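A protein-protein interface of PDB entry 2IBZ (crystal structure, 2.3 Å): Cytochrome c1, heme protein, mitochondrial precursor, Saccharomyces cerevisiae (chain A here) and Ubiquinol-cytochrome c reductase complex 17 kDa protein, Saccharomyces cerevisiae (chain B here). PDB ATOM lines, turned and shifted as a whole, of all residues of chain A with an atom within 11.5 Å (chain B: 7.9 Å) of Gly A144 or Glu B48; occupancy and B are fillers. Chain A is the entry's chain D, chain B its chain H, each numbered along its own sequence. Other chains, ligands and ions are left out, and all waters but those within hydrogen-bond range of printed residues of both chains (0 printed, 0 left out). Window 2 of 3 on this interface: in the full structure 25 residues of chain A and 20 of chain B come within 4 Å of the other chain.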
ATOM      1  N   ALA A   4     -20.069 -11.090  -9.461  1.00  0.00           N
ATOM      2  CA  ALA A   4     -21.263 -11.808  -9.026  1.00  0.00           C
ATOM      3  C   ALA A   4     -21.682 -12.835 -10.065  1.00  0.00           C
ATOM      4  O   ALA A   4     -22.024 -13.967  -9.728  1.00  0.00           O
ATOM      5  CB  ALA A   4     -22.402 -10.830  -8.767  1.00  0.00           C
ATOM      6  N   GLU A 140     -26.959 -14.010   5.946  1.00  0.00           N
ATOM      7  CA  GLU A 140     -27.702 -12.967   5.250  1.00  0.00           C
ATOM      8  C   GLU A 140     -26.944 -12.531   3.992  1.00  0.00           C
ATOM      9  O   GLU A 140     -25.719 -12.442   4.006  1.00  0.00           O
ATOM     10  CB  GLU A 140     -27.920 -11.762   6.177  1.00  0.00           C
ATOM     11  CG  GLU A 140     -29.056 -11.943   7.192  1.00  0.00           C
ATOM     12  CD  GLU A 140     -29.114 -10.829   8.229  1.00  0.00           C
ATOM     13  OE1 GLU A 140     -29.521  -9.696   7.877  1.00  0.00           O
ATOM     14  OE2 GLU A 140     -28.757 -11.096   9.404  1.00  0.00           O
ATOM     15  N   PRO A 141     -27.660 -12.307   2.873  1.00  0.00           N
ATOM     16  CA  PRO A 141     -27.033 -11.879   1.616  1.00  0.00           C
ATOM     17  C   PRO A 141     -26.474 -10.460   1.730  1.00  0.00           C
ATOM     18  O   PRO A 141     -26.988  -9.653   2.503  1.00  0.00           O
ATOM     19  CB  PRO A 141     -28.196 -11.937   0.623  1.00  0.00           C
ATOM     20  CG  PRO A 141     -29.388 -11.663   1.476  1.00  0.00           C
ATOM     21  CD  PRO A 141     -29.106 -12.517   2.682  1.00  0.00           C
ATOM     22  N   PRO A 142     -25.412 -10.138   0.964  1.00  0.00           N
ATOM     23  CA  PRO A 142     -24.827  -8.795   1.021  1.00  0.00           C
ATOM     24  C   PRO A 142     -25.857  -7.716   0.691  1.00  0.00           C
ATOM     25  O   PRO A 142     -26.769  -7.931  -0.111  1.00  0.00           O
ATOM     26  CB  PRO A 142     -23.697  -8.867  -0.014  1.00  0.00           C
ATOM     27  CG  PRO A 142     -24.174  -9.895  -0.975  1.00  0.00           C
ATOM     28  CD  PRO A 142     -24.737 -10.951  -0.063  1.00  0.00           C
ATOM     29  N   ALA A 143     -25.707  -6.567   1.339  1.00  0.00           N
ATOM     30  CA  ALA A 143     -26.615  -5.439   1.175  1.00  0.00           C
ATOM     31  C   ALA A 143     -26.905  -5.046  -0.269  1.00  0.00           C
ATOM     32  O   ALA A 143     -25.991  -4.880  -1.069  1.00  0.00           O
ATOM     33  CB  ALA A 143     -26.084  -4.242   1.946  1.00  0.00           C
ATOM     34  N   GLY A 144     -28.190  -4.905  -0.587  1.00  0.00           N
ATOM     35  CA  GLY A 144     -28.590  -4.506  -1.924  1.00  0.00           C
ATOM     36  C   GLY A 144     -29.014  -5.639  -2.829  1.00  0.00           C
ATOM     37  O   GLY A 144     -29.698  -5.418  -3.830  1.00  0.00           O
ATOM     38  N   VAL A 145     -28.606  -6.855  -2.488  1.00  0.00           N
ATOM     39  CA  VAL A 145     -28.954  -8.018  -3.287  1.00  0.00           C
ATOM     40  C   VAL A 145     -30.424  -8.395  -3.104  1.00  0.00           C
ATOM     41  O   VAL A 145     -30.862  -8.750  -2.004  1.00  0.00           O
ATOM     42  CB  VAL A 145     -28.042  -9.218  -2.962  1.00  0.00           C
ATOM     43  CG1 VAL A 145     -28.448 -10.425  -3.782  1.00  0.00           C
ATOM     44  CG2 VAL A 145     -26.601  -8.861  -3.253  1.00  0.00           C
ATOM     45  N   ALA A 146     -31.180  -8.259  -4.189  1.00  0.00           N
ATOM     46  CA  ALA A 146     -32.601  -8.584  -4.206  1.00  0.00           C
ATOM     47  C   ALA A 146     -32.740 -10.045  -4.606  1.00  0.00           C
ATOM     48  O   ALA A 146     -32.764 -10.385  -5.793  1.00  0.00           O
ATOM     49  CB  ALA A 146     -33.337  -7.683  -5.197  1.00  0.00           C
ATOM     50  N   LEU A 147     -32.822 -10.903  -3.596  1.00  0.00           N
ATOM     51  CA  LEU A 147     -32.932 -12.341  -3.793  1.00  0.00           C
ATOM     52  C   LEU A 147     -34.371 -12.787  -4.049  1.00  0.00           C
ATOM     53  O   LEU A 147     -35.247 -12.582  -3.206  1.00  0.00           O
ATOM     54  CB  LEU A 147     -32.382 -13.048  -2.558  1.00  0.00           C
ATOM     55  CG  LEU A 147     -31.835 -14.461  -2.721  1.00  0.00           C
ATOM     56  CD1 LEU A 147     -30.668 -14.462  -3.712  1.00  0.00           C
ATOM     57  CD2 LEU A 147     -31.387 -14.959  -1.358  1.00  0.00           C
ATOM     58  N   PRO A 148     -34.629 -13.421  -5.210  1.00  0.00           N
ATOM     59  CA  PRO A 148     -35.964 -13.906  -5.586  1.00  0.00           C
ATOM     60  C   PRO A 148     -36.557 -14.858  -4.540  1.00  0.00           C
ATOM     61  O   PRO A 148     -35.824 -15.510  -3.790  1.00  0.00           O
ATOM     62  CB  PRO A 148     -35.700 -14.640  -6.902  1.00  0.00           C
ATOM     63  CG  PRO A 148     -34.549 -13.896  -7.481  1.00  0.00           C
ATOM     64  CD  PRO A 148     -33.656 -13.714  -6.277  1.00  0.00           C
ATOM     65  N   TYR A 153     -28.850 -17.331  -1.272  1.00  0.00           N
ATOM     66  CA  TYR A 153     -27.619 -16.717  -1.711  1.00  0.00           C
ATOM     67  C   TYR A 153     -26.416 -17.553  -1.310  1.00  0.00           C
ATOM     68  O   TYR A 153     -26.367 -18.112  -0.214  1.00  0.00           O
ATOM     69  CB  TYR A 153     -27.479 -15.299  -1.159  1.00  0.00           C
ATOM     70  CG  TYR A 153     -26.228 -14.598  -1.637  1.00  0.00           C
ATOM     71  CD1 TYR A 153     -26.218 -13.892  -2.838  1.00  0.00           C
ATOM     72  CD2 TYR A 153     -25.045 -14.672  -0.905  1.00  0.00           C
ATOM     73  CE1 TYR A 153     -25.059 -13.278  -3.301  1.00  0.00           C
ATOM     74  CE2 TYR A 153     -23.879 -14.070  -1.358  1.00  0.00           C
ATOM     75  CZ  TYR A 153     -23.897 -13.377  -2.555  1.00  0.00           C
ATOM     76  OH  TYR A 153     -22.750 -12.781  -2.996  1.00  0.00           O
ATOM     77  N   GLY A 159     -23.799 -16.167 -10.320  1.00  0.00           N
ATOM     78  CA  GLY A 159     -25.034 -15.404 -10.217  1.00  0.00           C
ATOM     79  C   GLY A 159     -25.537 -15.259  -8.783  1.00  0.00           C
ATOM     80  O   GLY A 159     -26.526 -14.559  -8.540  1.00  0.00           O
ATOM     81  N   SER A 161     -27.508 -16.635  -6.878  1.00  0.00           N
ATOM     82  CA  SER A 161     -28.819 -17.155  -6.531  1.00  0.00           C
ATOM     83  C   SER A 161     -28.967 -18.656  -6.823  1.00  0.00           C
ATOM     84  O   SER A 161     -29.170 -19.063  -7.968  1.00  0.00           O
ATOM     85  CB  SER A 161     -29.885 -16.336  -7.258  1.00  0.00           C
ATOM     86  OG  SER A 161     -31.175 -16.866  -7.046  1.00  0.00           O
ATOM     87  N   TYR B  25     -16.946  -2.986   3.782  1.00  0.00           N
ATOM     88  CA  TYR B  25     -18.190  -3.661   3.439  1.00  0.00           C
ATOM     89  C   TYR B  25     -19.314  -2.987   4.215  1.00  0.00           C
ATOM     90  O   TYR B  25     -20.407  -2.769   3.684  1.00  0.00           O
ATOM     91  CB  TYR B  25     -18.150  -5.166   3.774  1.00  0.00           C
ATOM     92  CG  TYR B  25     -19.523  -5.801   3.686  1.00  0.00           C
ATOM     93  CD1 TYR B  25     -20.156  -5.950   2.457  1.00  0.00           C
ATOM     94  CD2 TYR B  25     -20.254  -6.098   4.840  1.00  0.00           C
ATOM     95  CE1 TYR B  25     -21.477  -6.354   2.368  1.00  0.00           C
ATOM     96  CE2 TYR B  25     -21.591  -6.508   4.764  1.00  0.00           C
ATOM     97  CZ  TYR B  25     -22.194  -6.627   3.520  1.00  0.00           C
ATOM     98  OH  TYR B  25     -23.524  -6.974   3.421  1.00  0.00           O
ATOM     99  N   GLU B  27     -19.360   0.157   5.460  1.00  0.00           N
ATOM    100  CA  GLU B  27     -19.577   1.501   4.938  1.00  0.00           C
ATOM    101  C   GLU B  27     -20.443   1.437   3.677  1.00  0.00           C
ATOM    102  O   GLU B  27     -21.164   2.387   3.362  1.00  0.00           O
ATOM    103  CB  GLU B  27     -18.238   2.183   4.644  1.00  0.00           C
ATOM    104  CG  GLU B  27     -18.349   3.679   4.371  1.00  0.00           C
ATOM    105  CD  GLU B  27     -17.007   4.400   4.462  1.00  0.00           C
ATOM    106  OE1 GLU B  27     -16.277   4.442   3.442  1.00  0.00           O
ATOM    107  OE2 GLU B  27     -16.687   4.925   5.557  1.00  0.00           O
ATOM    108  N   CYS B  28     -20.381   0.302   2.973  1.00  0.00           N
ATOM    109  CA  CYS B  28     -21.176   0.101   1.768  1.00  0.00           C
ATOM    110  C   CYS B  28     -22.611  -0.234   2.153  1.00  0.00           C
ATOM    111  O   CYS B  28     -23.551   0.309   1.580  1.00  0.00           O
ATOM    112  CB  CYS B  28     -20.599  -1.029   0.901  1.00  0.00           C
ATOM    113  SG  CYS B  28     -21.489  -1.289  -0.678  1.00  0.00           S
ATOM    114  N   ALA B  29     -22.763  -1.135   3.123  1.00  0.00           N
ATOM    115  CA  ALA B  29     -24.076  -1.565   3.604  1.00  0.00           C
ATOM    116  C   ALA B  29     -24.898  -0.394   4.145  1.00  0.00           C
ATOM    117  O   ALA B  29     -26.112  -0.312   3.928  1.00  0.00           O
ATOM    118  CB  ALA B  29     -23.915  -2.639   4.674  1.00  0.00           C
ATOM    119  N   ARG B  31     -24.551   2.871   3.333  1.00  0.00           N
ATOM    120  CA  ARG B  31     -24.914   3.675   2.173  1.00  0.00           C
ATOM    121  C   ARG B  31     -26.107   3.100   1.405  1.00  0.00           C
ATOM    122  O   ARG B  31     -26.937   3.845   0.888  1.00  0.00           O
ATOM    123  CB  ARG B  31     -23.691   3.818   1.259  1.00  0.00           C
ATOM    124  CG  ARG B  31     -23.899   4.685   0.028  1.00  0.00           C
ATOM    125  CD  ARG B  31     -22.575   5.013  -0.669  1.00  0.00           C
ATOM    126  NE  ARG B  31     -21.886   3.833  -1.194  1.00  0.00           N
ATOM    127  CZ  ARG B  31     -20.745   3.346  -0.705  1.00  0.00           C
ATOM    128  NH1 ARG B  31     -20.192   2.270  -1.252  1.00  0.00           N
ATOM    129  NH2 ARG B  31     -20.160   3.928   0.336  1.00  0.00           N
ATOM    130  N   VAL B  32     -26.225   1.776   1.391  1.00  0.00           N
ATOM    131  CA  VAL B  32     -27.309   1.105   0.681  1.00  0.00           C
ATOM    132  C   VAL B  32     -28.687   1.242   1.326  1.00  0.00           C
ATOM    133  O   VAL B  32     -29.647   1.600   0.643  1.00  0.00           O
ATOM    134  CB  VAL B  32     -26.987  -0.390   0.441  1.00  0.00           C
ATOM    135  CG1 VAL B  32     -28.159  -1.094  -0.232  1.00  0.00           C
ATOM    136  CG2 VAL B  32     -25.756  -0.516  -0.427  1.00  0.00           C
ATOM    137  N   LYS B  33     -28.796   0.963   2.625  1.00  0.00           N
ATOM    138  CA  LYS B  33     -30.095   1.063   3.302  1.00  0.00           C
ATOM    139  C   LYS B  33     -30.640   2.490   3.317  1.00  0.00           C
ATOM    140  O   LYS B  33     -31.851   2.698   3.358  1.00  0.00           O
ATOM    141  CB  LYS B  33     -30.043   0.489   4.726  1.00  0.00           C
ATOM    142  CG  LYS B  33     -29.232   1.292   5.731  1.00  0.00           C
ATOM    143  CD  LYS B  33     -29.461   0.769   7.146  1.00  0.00           C
ATOM    144  CE  LYS B  33     -28.549   1.447   8.169  1.00  0.00           C
ATOM    145  NZ  LYS B  33     -27.100   1.120   7.977  1.00  0.00           N
ATOM    146  N   GLN B  35     -30.369   4.506   0.852  1.00  0.00           N
ATOM    147  CA  GLN B  35     -30.919   4.723  -0.483  1.00  0.00           C
ATOM    148  C   GLN B  35     -32.269   4.027  -0.665  1.00  0.00           C
ATOM    149  O   GLN B  35     -33.080   4.443  -1.493  1.00  0.00           O
ATOM    150  CB  GLN B  35     -29.946   4.220  -1.553  1.00  0.00           C
ATOM    151  CG  GLN B  35     -28.603   4.934  -1.592  1.00  0.00           C
ATOM    152  CD  GLN B  35     -27.680   4.393  -2.676  1.00  0.00           C
ATOM    153  OE1 GLN B  35     -28.078   3.556  -3.491  1.00  0.00           O
ATOM    154  NE2 GLN B  35     -26.442   4.872  -2.689  1.00  0.00           N
ATOM    155  N   GLN B  36     -32.494   2.963   0.104  1.00  0.00           N
ATOM    156  CA  GLN B  36     -33.736   2.191   0.030  1.00  0.00           C
ATOM    157  C   GLN B  36     -34.922   2.899   0.678  1.00  0.00           C
ATOM    158  O   GLN B  36     -36.055   2.794   0.203  1.00  0.00           O
ATOM    159  CB  GLN B  36     -33.549   0.817   0.679  1.00  0.00           C
ATOM    160  CG  GLN B  36     -32.422  -0.010   0.083  1.00  0.00           C
ATOM    161  CD  GLN B  36     -32.365  -1.418   0.641  1.00  0.00           C
ATOM    162  OE1 GLN B  36     -32.070  -2.370  -0.082  1.00  0.00           O
ATOM    163  NE2 GLN B  36     -32.650  -1.561   1.931  1.00  0.00           N
ATOM    164  N   TYR B  41     -37.179   4.246  -4.965  1.00  0.00           N
ATOM    165  CA  TYR B  41     -36.168   3.196  -4.985  1.00  0.00           C
ATOM    166  C   TYR B  41     -36.557   2.062  -5.927  1.00  0.00           C
ATOM    167  O   TYR B  41     -35.693   1.443  -6.547  1.00  0.00           O
ATOM    168  CB  TYR B  41     -35.921   2.642  -3.580  1.00  0.00           C
ATOM    169  CG  TYR B  41     -34.868   1.555  -3.538  1.00  0.00           C
ATOM    170  CD1 TYR B  41     -35.218   0.229  -3.279  1.00  0.00           C
ATOM    171  CD2 TYR B  41     -33.525   1.845  -3.781  1.00  0.00           C
ATOM    172  CE1 TYR B  41     -34.258  -0.781  -3.267  1.00  0.00           C
ATOM    173  CE2 TYR B  41     -32.557   0.843  -3.769  1.00  0.00           C
ATOM    174  CZ  TYR B  41     -32.931  -0.468  -3.512  1.00  0.00           C
ATOM    175  OH  TYR B  41     -31.982  -1.465  -3.498  1.00  0.00           O
ATOM    176  N   LEU B  44     -35.474   2.826 -10.218  1.00  0.00           N
ATOM    177  CA  LEU B  44     -34.202   3.541 -10.210  1.00  0.00           C
ATOM    178  C   LEU B  44     -33.206   3.007 -11.240  1.00  0.00           C
ATOM    179  O   LEU B  44     -32.363   3.761 -11.730  1.00  0.00           O
ATOM    180  CB  LEU B  44     -33.579   3.485  -8.810  1.00  0.00           C
ATOM    181  CG  LEU B  44     -33.076   4.788  -8.176  1.00  0.00           C
ATOM    182  CD1 LEU B  44     -32.572   4.503  -6.773  1.00  0.00           C
ATOM    183  CD2 LEU B  44     -31.979   5.419  -9.012  1.00  0.00           C
ATOM    184  N   GLU B  45     -33.313   1.717 -11.566  1.00  0.00           N
ATOM    185  CA  GLU B  45     -32.426   1.035 -12.525  1.00  0.00           C
ATOM    186  C   GLU B  45     -30.944   1.393 -12.350  1.00  0.00           C
ATOM    187  O   GLU B  45     -30.161   1.343 -13.303  1.00  0.00           O
ATOM    188  CB  GLU B  45     -32.866   1.279 -13.981  1.00  0.00           C
ATOM    189  CG  GLU B  45     -32.688   2.712 -14.498  1.00  0.00           C
ATOM    190  CD  GLU B  45     -32.568   2.795 -16.014  1.00  0.00           C
ATOM    191  OE1 GLU B  45     -33.268   2.040 -16.724  1.00  0.00           O
ATOM    192  OE2 GLU B  45     -31.765   3.622 -16.495  1.00  0.00           O
ATOM    193  N   HIS B  46     -30.567   1.719 -11.118  1.00  0.00           N
ATOM    194  CA  HIS B  46     -29.198   2.105 -10.793  1.00  0.00           C
ATOM    195  C   HIS B  46     -28.920   1.752  -9.328  1.00  0.00           C
ATOM    196  O   HIS B  46     -28.106   2.398  -8.663  1.00  0.00           O
ATOM    197  CB  HIS B  46     -29.035   3.615 -11.009  1.00  0.00           C
ATOM    198  CG  HIS B  46     -27.720   4.010 -11.605  1.00  0.00           C
ATOM    199  ND1 HIS B  46     -26.629   4.358 -10.838  1.00  0.00           N
ATOM    200  CD2 HIS B  46     -27.330   4.141 -12.895  1.00  0.00           C
ATOM    201  CE1 HIS B  46     -25.624   4.689 -11.630  1.00  0.00           C
ATOM    202  NE2 HIS B  46     -26.024   4.567 -12.883  1.00  0.00           N
ATOM    203  N   LYS B  47     -29.603   0.718  -8.839  1.00  0.00           N
ATOM    204  CA  LYS B  47     -29.467   0.259  -7.459  1.00  0.00           C
ATOM    205  C   LYS B  47     -28.089  -0.340  -7.199  1.00  0.00           C
ATOM    206  O   LYS B  47     -27.626  -1.213  -7.933  1.00  0.00           O
ATOM    207  CB  LYS B  47     -30.544  -0.780  -7.129  1.00  0.00           C
ATOM    208  CG  LYS B  47     -31.938  -0.431  -7.637  1.00  0.00           C
ATOM    209  CD  LYS B  47     -32.950  -1.504  -7.260  1.00  0.00           C
ATOM    210  CE  LYS B  47     -34.107  -1.558  -8.255  1.00  0.00           C
ATOM    211  NZ  LYS B  47     -34.808  -0.255  -8.407  1.00  0.00           N
ATOM    212  N   GLU B  48     -27.437   0.144  -6.150  1.00  0.00           N
ATOM    213  CA  GLU B  48     -26.117  -0.334  -5.782  1.00  0.00           C
ATOM    214  C   GLU B  48     -26.207  -1.480  -4.779  1.00  0.00           C
ATOM    215  O   GLU B  48     -27.099  -1.502  -3.927  1.00  0.00           O
ATOM    216  CB  GLU B  48     -25.295   0.810  -5.183  1.00  0.00           C
ATOM    217  CG  GLU B  48     -23.893   0.409  -4.728  1.00  0.00           C
ATOM    218  CD  GLU B  48     -23.121   1.549  -4.079  1.00  0.00           C
ATOM    219  OE1 GLU B  48     -23.735   2.585  -3.747  1.00  0.00           O
ATOM    220  OE2 GLU B  48     -21.893   1.406  -3.893  1.00  0.00           O
ATOM    221  N   ASP B  49     -25.313  -2.455  -4.926  1.00  0.00           N
ATOM    222  CA  ASP B  49     -25.249  -3.587  -4.011  1.00  0.00           C
ATOM    223  C   ASP B  49     -23.831  -3.645  -3.472  1.00  0.00           C
ATOM    224  O   ASP B  49     -22.962  -2.921  -3.942  1.00  0.00           O
ATOM    225  CB  ASP B  49     -25.658  -4.905  -4.685  1.00  0.00           C
ATOM    226  CG  ASP B  49     -24.773  -5.277  -5.860  1.00  0.00           C
ATOM    227  OD1 ASP B  49     -25.312  -5.333  -6.988  1.00  0.00           O
ATOM    228  OD2 ASP B  49     -23.561  -5.537  -5.662  1.00  0.00           O
ATOM    229  N   CYS B  50     -23.589  -4.510  -2.498  1.00  0.00           N
ATOM    230  CA  CYS B  50     -22.267  -4.595  -1.900  1.00  0.00           C
ATOM    231  C   CYS B  50     -21.548  -5.938  -2.097  1.00  0.00           C
ATOM    232  O   CYS B  50     -20.683  -6.324  -1.292  1.00  0.00           O
ATOM    233  CB  CYS B  50     -22.363  -4.199  -0.420  1.00  0.00           C
ATOM    234  SG  CYS B  50     -23.040  -2.514  -0.186  1.00  0.00           S
ATOM    235  N   VAL B  51     -21.865  -6.602  -3.214  1.00  0.00           N
ATOM    236  CA  VAL B  51     -21.268  -7.892  -3.563  1.00  0.00           C
ATOM    237  C   VAL B  51     -19.752  -7.774  -3.679  1.00  0.00           C
ATOM    238  O   VAL B  51     -19.011  -8.554  -3.092  1.00  0.00           O
ATOM    239  CB  VAL B  51     -21.839  -8.436  -4.893  1.00  0.00           C
ATOM    240  CG1 VAL B  51     -21.177  -9.757  -5.251  1.00  0.00           C
ATOM    241  CG2 VAL B  51     -23.327  -8.639  -4.785  1.00  0.00           C
ATOM    242  N   GLU B  53     -17.634  -5.529  -2.397  1.00  0.00           N
ATOM    243  CA  GLU B  53     -17.030  -5.344  -1.075  1.00  0.00           C
ATOM    244  C   GLU B  53     -17.101  -6.651  -0.289  1.00  0.00           C
ATOM    245  O   GLU B  53     -16.163  -7.006   0.427  1.00  0.00           O
ATOM    246  CB  GLU B  53     -17.735  -4.228  -0.296  1.00  0.00           C
ATOM    247  CG  GLU B  53     -17.494  -2.816  -0.830  1.00  0.00           C
ATOM    248  CD  GLU B  53     -18.296  -2.499  -2.081  1.00  0.00           C
ATOM    249  OE1 GLU B  53     -19.256  -3.241  -2.394  1.00  0.00           O
ATOM    250  OE2 GLU B  53     -17.972  -1.493  -2.746  1.00  0.00           O
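The backbone NH of Ala A143 sits at hydrogen-bond distance from the side-chain hydroxyl of Tyr B25 (3.0 Å). The backbone carbonyl oxygen (O) of Ala A143 sits at hydrogen-bond distance from the backbone NH (N) of Cys B50.
The backbone carbonyl oxygen of Ala A4 lies within hydrogen-bond range of the backbone NH of Gly A159 (2.9 Å). The side-chain sulfur (SG) of Cys B50 forms a disulfide with the side-chain sulfur (SG) of Cys B28, 2.0 Å away. The backbone NH (N) of Ala B29 sits at hydrogen-bond distance from the side-chain sulfur (SG) of Cys B50 (3.6 Å). The guanidinium group (NH1) of Arg B31 lies within salt-bridge range of the side-chain carboxylate (OE2) of Glu B48 (3.3 Å). The side-chain carboxylate (OD2) of Asp B49 sits at hydrogen-bond distance from the backbone NH (N) of Val B51 (3.2 Å).
Among the printed residues, merely in contact across the chains: Pro A142 with Tyr B25 (3.3 Å), Ala A143 with Asp B49 (3.3 Å), Val A145 with Val B51 (3.6 Å), Ala A143 with Ala B29 (3.7 Å), Gly A144 with Val B32 (3.8 Å), Ala A4 with Val B51 (3.9 Å), Gly A144 with Asp B49 (3.9 Å) and Gly A144 with Glu B48 (3.9 Å).
Of chain B, only Val B32 (3.8 Å), Glu B48 (3.9 Å) and Asp B49 (3.9 Å) come within 4 Å of Gly A144. No residue of chain A comes within 4 Å of Cys B28. No residue of chain A comes within 4 Å of Arg B31. Val B32 touches just one residue of chain A: Gly A144 (3.8 Å). Printed residues of chain A within 4 Å of Tyr B25: Pro A142 and Ala A143. Printed residues of chain B within 4 Å of Val A145: Val B51 (3.6 Å). The nearest residue of chain A that does not touch Glu B48 is Ala A143 (4.6 Å).
Hydrophobic or aromatic side chains of chain A that line the printed part of chain B: Ala A4, Pro A142, Ala A143 and Val A145. Among the printed residues, 10 pairs touch across the chains.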
